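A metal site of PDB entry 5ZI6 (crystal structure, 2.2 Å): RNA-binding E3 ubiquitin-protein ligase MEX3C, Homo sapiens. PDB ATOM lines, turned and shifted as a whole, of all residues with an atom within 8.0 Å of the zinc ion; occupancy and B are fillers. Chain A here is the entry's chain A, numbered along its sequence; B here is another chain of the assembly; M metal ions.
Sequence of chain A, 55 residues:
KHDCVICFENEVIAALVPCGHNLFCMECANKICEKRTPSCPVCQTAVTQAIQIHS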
ATOM      1  N   LEU A  16     -16.647  15.399 -18.477  1.00  0.00           N
ATOM      2  CA  LEU A  16     -15.347  14.795 -18.786  1.00  0.00           C
ATOM      3  C   LEU A  16     -15.480  13.300 -19.064  1.00  0.00           C
ATOM      4  O   LEU A  16     -16.341  12.599 -18.509  1.00  0.00           O
ATOM      5  CB  LEU A  16     -14.368  15.029 -17.644  1.00  0.00           C
ATOM      6  CG  LEU A  16     -14.210  16.479 -17.186  1.00  0.00           C
ATOM      7  CD1 LEU A  16     -13.290  16.538 -15.960  1.00  0.00           C
ATOM      8  CD2 LEU A  16     -13.669  17.355 -18.294  1.00  0.00           C
ATOM      9  N   VAL A  17     -14.605  12.802 -19.927  1.00  0.00           N
ATOM     10  CA  VAL A  17     -14.556  11.403 -20.303  1.00  0.00           C
ATOM     11  C   VAL A  17     -13.259  10.810 -19.792  1.00  0.00           C
ATOM     12  O   VAL A  17     -12.202  11.425 -19.950  1.00  0.00           O
ATOM     13  CB  VAL A  17     -14.647  11.219 -21.813  1.00  0.00           C
ATOM     14  CG1 VAL A  17     -14.680   9.744 -22.191  1.00  0.00           C
ATOM     15  CG2 VAL A  17     -15.889  11.950 -22.341  1.00  0.00           C
ATOM     16  N   PRO A  18     -13.329   9.613 -19.172  1.00  0.00           N
ATOM     17  CA  PRO A  18     -14.531   8.799 -19.011  1.00  0.00           C
ATOM     18  C   PRO A  18     -15.266   8.910 -17.667  1.00  0.00           C
ATOM     19  O   PRO A  18     -16.282   8.244 -17.547  1.00  0.00           O
ATOM     20  CB  PRO A  18     -13.981   7.380 -19.172  1.00  0.00           C
ATOM     21  CG  PRO A  18     -12.664   7.462 -18.461  1.00  0.00           C
ATOM     22  CD  PRO A  18     -12.128   8.870 -18.749  1.00  0.00           C
ATOM     23  N   CYS A  19     -14.813   9.732 -16.709  1.00  0.00           N
ATOM     24  CA  CYS A  19     -15.476   9.741 -15.403  1.00  0.00           C
ATOM     25  C   CYS A  19     -16.925  10.228 -15.460  1.00  0.00           C
ATOM     26  O   CYS A  19     -17.710   9.894 -14.562  1.00  0.00           O
ATOM     27  CB  CYS A  19     -14.700  10.590 -14.372  1.00  0.00           C
ATOM     28  SG  CYS A  19     -14.706  12.412 -14.568  1.00  0.00           S
ATOM     29  N   GLY A  20     -17.289  11.010 -16.492  1.00  0.00           N
ATOM     30  CA  GLY A  20     -18.663  11.446 -16.683  1.00  0.00           C
ATOM     31  C   GLY A  20     -19.099  12.588 -15.784  1.00  0.00           C
ATOM     32  O   GLY A  20     -20.296  12.899 -15.728  1.00  0.00           O
ATOM     33  N   HIS A  21     -18.176  13.223 -15.069  1.00  0.00           N
ATOM     34  CA  HIS A  21     -18.551  14.360 -14.242  1.00  0.00           C
ATOM     35  C   HIS A  21     -19.012  15.511 -15.119  1.00  0.00           C
ATOM     36  O   HIS A  21     -18.297  15.939 -16.029  1.00  0.00           O
ATOM     37  CB  HIS A  21     -17.409  14.767 -13.307  1.00  0.00           C
ATOM     38  CG  HIS A  21     -17.447  14.034 -12.005  1.00  0.00           C
ATOM     39  ND1 HIS A  21     -16.415  13.222 -11.570  1.00  0.00           N
ATOM     40  CD2 HIS A  21     -18.423  13.916 -11.075  1.00  0.00           C
ATOM     41  CE1 HIS A  21     -16.748  12.665 -10.424  1.00  0.00           C
ATOM     42  NE2 HIS A  21     -17.962  13.071 -10.098  1.00  0.00           N
ATOM     43  N   ASN A  22     -20.252  15.929 -14.893  1.00  0.00           N
ATOM     44  CA  ASN A  22     -20.961  16.892 -15.722  1.00  0.00           C
ATOM     45  C   ASN A  22     -21.208  18.120 -14.858  1.00  0.00           C
ATOM     46  O   ASN A  22     -22.320  18.367 -14.387  1.00  0.00           O
ATOM     47  CB  ASN A  22     -22.282  16.219 -16.242  1.00  0.00           C
ATOM     48  CG  ASN A  22     -23.167  17.166 -17.057  1.00  0.00           C
ATOM     49  OD1 ASN A  22     -22.705  18.045 -17.796  1.00  0.00           O
ATOM     50  ND2 ASN A  22     -24.468  16.963 -16.933  1.00  0.00           N
ATOM     51  N   LEU A  23     -20.113  18.874 -14.632  1.00  0.00           N
ATOM     52  CA  LEU A  23     -20.075  19.958 -13.653  1.00  0.00           C
ATOM     53  C   LEU A  23     -19.306  21.176 -14.175  1.00  0.00           C
ATOM     54  O   LEU A  23     -18.825  21.979 -13.364  1.00  0.00           O
ATOM     55  CB  LEU A  23     -19.422  19.473 -12.357  1.00  0.00           C
ATOM     56  CG  LEU A  23     -20.201  18.378 -11.637  1.00  0.00           C
ATOM     57  CD1 LEU A  23     -19.378  17.737 -10.512  1.00  0.00           C
ATOM     58  CD2 LEU A  23     -21.469  18.981 -11.098  1.00  0.00           C
ATOM     59  N   PHE A  24     -19.133  21.292 -15.479  1.00  0.00           N
ATOM     60  CA  PHE A  24     -18.192  22.267 -16.012  1.00  0.00           C
ATOM     61  C   PHE A  24     -18.840  23.043 -17.158  1.00  0.00           C
ATOM     62  O   PHE A  24     -19.655  22.504 -17.918  1.00  0.00           O
ATOM     63  CB  PHE A  24     -16.904  21.556 -16.492  1.00  0.00           C
ATOM     64  CG  PHE A  24     -16.353  20.561 -15.499  1.00  0.00           C
ATOM     65  CD1 PHE A  24     -15.649  20.993 -14.395  1.00  0.00           C
ATOM     66  CD2 PHE A  24     -16.592  19.196 -15.656  1.00  0.00           C
ATOM     67  CE1 PHE A  24     -15.168  20.075 -13.446  1.00  0.00           C
ATOM     68  CE2 PHE A  24     -16.112  18.273 -14.720  1.00  0.00           C
ATOM     69  CZ  PHE A  24     -15.393  18.720 -13.615  1.00  0.00           C
ATOM     70  N   SER A  39      -6.735  15.815 -15.662  1.00  0.00           N
ATOM     71  CA  SER A  39      -7.470  14.962 -14.747  1.00  0.00           C
ATOM     72  C   SER A  39      -8.655  15.736 -14.187  1.00  0.00           C
ATOM     73  O   SER A  39      -8.592  16.948 -13.997  1.00  0.00           O
ATOM     74  CB  SER A  39      -6.583  14.410 -13.630  1.00  0.00           C
ATOM     75  OG  SER A  39      -6.184  15.444 -12.766  1.00  0.00           O
ATOM     76  N   CYS A  40      -9.707  14.999 -13.865  1.00  0.00           N
ATOM     77  CA  CYS A  40     -10.910  15.596 -13.330  1.00  0.00           C
ATOM     78  C   CYS A  40     -10.608  16.196 -11.960  1.00  0.00           C
ATOM     79  O   CYS A  40     -10.092  15.491 -11.091  1.00  0.00           O
ATOM     80  CB  CYS A  40     -12.011  14.544 -13.198  1.00  0.00           C
ATOM     81  SG  CYS A  40     -13.499  15.081 -12.289  1.00  0.00           S
ATOM     82  N   PRO A  41     -10.879  17.483 -11.734  1.00  0.00           N
ATOM     83  CA  PRO A  41     -10.652  18.057 -10.393  1.00  0.00           C
ATOM     84  C   PRO A  41     -11.538  17.472  -9.288  1.00  0.00           C
ATOM     85  O   PRO A  41     -11.207  17.632  -8.102  1.00  0.00           O
ATOM     86  CB  PRO A  41     -10.922  19.553 -10.597  1.00  0.00           C
ATOM     87  CG  PRO A  41     -11.676  19.658 -11.837  1.00  0.00           C
ATOM     88  CD  PRO A  41     -11.321  18.492 -12.704  1.00  0.00           C
ATOM     89  N   VAL A  42     -12.606  16.764  -9.609  1.00  0.00           N
ATOM     90  CA  VAL A  42     -13.490  16.224  -8.566  1.00  0.00           C
ATOM     91  C   VAL A  42     -13.053  14.837  -8.123  1.00  0.00           C
ATOM     92  O   VAL A  42     -13.014  14.542  -6.934  1.00  0.00           O
ATOM     93  CB  VAL A  42     -14.963  16.250  -9.029  1.00  0.00           C
ATOM     94  CG1 VAL A  42     -15.850  15.562  -7.993  1.00  0.00           C
ATOM     95  CG2 VAL A  42     -15.419  17.690  -9.233  1.00  0.00           C
ATOM     96  N   CYS A  43     -12.799  13.911  -9.052  1.00  0.00           N
ATOM     97  CA  CYS A  43     -12.482  12.550  -8.667  1.00  0.00           C
ATOM     98  C   CYS A  43     -11.056  12.139  -9.019  1.00  0.00           C
ATOM     99  O   CYS A  43     -10.685  10.986  -8.783  1.00  0.00           O
ATOM    100  CB  CYS A  43     -13.492  11.573  -9.303  1.00  0.00           C
ATOM    101  SG  CYS A  43     -13.329  11.458 -11.067  1.00  0.00           S
ATOM    102  N   GLN A  44     -10.256  13.024  -9.597  1.00  0.00           N
ATOM    103  CA  GLN A  44      -8.854  12.784  -9.933  1.00  0.00           C
ATOM    104  C   GLN A  44      -8.639  11.781 -11.056  1.00  0.00           C
ATOM    105  O   GLN A  44      -7.498  11.404 -11.318  1.00  0.00           O
ATOM    106  CB  GLN A  44      -8.041  12.321  -8.712  1.00  0.00           C
ATOM    107  CG  GLN A  44      -7.835  13.385  -7.644  1.00  0.00           C
ATOM    108  CD  GLN A  44      -9.089  13.642  -6.823  1.00  0.00           C
ATOM    109  OE1 GLN A  44      -9.656  12.730  -6.220  1.00  0.00           O
ATOM    110  NE2 GLN A  44      -9.536  14.902  -6.796  1.00  0.00           N
ATOM    111  N   THR A  45      -9.699  11.338 -11.737  1.00  0.00           N
ATOM    112  CA  THR A  45      -9.547  10.436 -12.883  1.00  0.00           C
ATOM    113  C   THR A  45      -8.899  11.148 -14.071  1.00  0.00           C
ATOM    114  O   THR A  45      -9.191  12.317 -14.366  1.00  0.00           O
ATOM    115  CB  THR A  45     -10.923   9.897 -13.288  1.00  0.00           C
ATOM    116  OG1 THR A  45     -11.467   9.129 -12.211  1.00  0.00           O
ATOM    117  CG2 THR A  45     -10.835   8.994 -14.526  1.00  0.00           C
ATOM    118  N   ALA A  46      -8.013  10.416 -14.776  1.00  0.00           N
ATOM    119  CA  ALA A  46      -7.413  10.932 -16.009  1.00  0.00           C
ATOM    120  C   ALA A  46      -8.490  11.187 -17.046  1.00  0.00           C
ATOM    121  O   ALA A  46      -9.415  10.387 -17.219  1.00  0.00           O
ATOM    122  CB  ALA A  46      -6.391   9.945 -16.567  1.00  0.00           C
ATOM    123  N   VAL A  47      -8.312  12.253 -17.825  1.00  0.00           N
ATOM    124  CA  VAL A  47      -9.327  12.739 -18.748  1.00  0.00           C
ATOM    125  C   VAL A  47      -8.826  12.534 -20.171  1.00  0.00           C
ATOM    126  O   VAL A  47      -7.751  13.006 -20.529  1.00  0.00           O
ATOM    127  CB  VAL A  47      -9.619  14.232 -18.480  1.00  0.00           C
ATOM    128  CG1 VAL A  47     -10.491  14.826 -19.561  1.00  0.00           C
ATOM    129  CG2 VAL A  47     -10.255  14.432 -17.087  1.00  0.00           C
ATOM    130  N   HIS B  54     -22.479  12.029 -14.085  1.00  0.00           N
ATOM    131  CA  HIS B  54     -22.535  12.353 -12.665  1.00  0.00           C
ATOM    132  C   HIS B  54     -22.643  13.862 -12.519  1.00  0.00           C
ATOM    133  O   HIS B  54     -21.719  14.594 -12.888  1.00  0.00           O
ATOM    134  CB  HIS B  54     -21.309  11.791 -11.939  1.00  0.00           C
ATOM    135  CG  HIS B  54     -21.247  10.295 -11.979  1.00  0.00           C
ATOM    136  ND1 HIS B  54     -20.399   9.615 -12.820  1.00  0.00           N
ATOM    137  CD2 HIS B  54     -21.989   9.353 -11.334  1.00  0.00           C
ATOM    138  CE1 HIS B  54     -20.578   8.314 -12.658  1.00  0.00           C
ATOM    139  NE2 HIS B  54     -21.552   8.132 -11.780  1.00  0.00           N
HETATM  140 ZN    ZN M   1     -14.571  13.043 -12.492  1.00  0.00          ZN
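The zinc ion is bound by ND1 of His 21 (2.1 Å). SG of Cys 19 is bound to the zinc ion (2.2 Å). The zinc ion is bound by SG of Cys 40. The zinc ion is bound by the side-chain sulfur (SG) of Cys 43 (2.5 Å). The zinc ion has four donor atoms within binding distance.
O of His 21 sits at hydrogen-bond distance from N of Leu 16 (3.0 Å). O of Cys 19 is in hydrogen-bond range of ND1 of His 54 of chain B, 3.2 Å away. SG of Cys 40 lies close to N of Val 42 (3.3 Å). O of Thr 45 is in hydrogen-bond range of N of Cys 40, 2.8 Å away. The side-chain sulfur (SG) of Cys 43 lies close to the side-chain hydroxyl (OG1) of Thr 45.
Within 4 Å of the zinc ion: Cys 19, His 21, Cys 40 and Cys 43.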
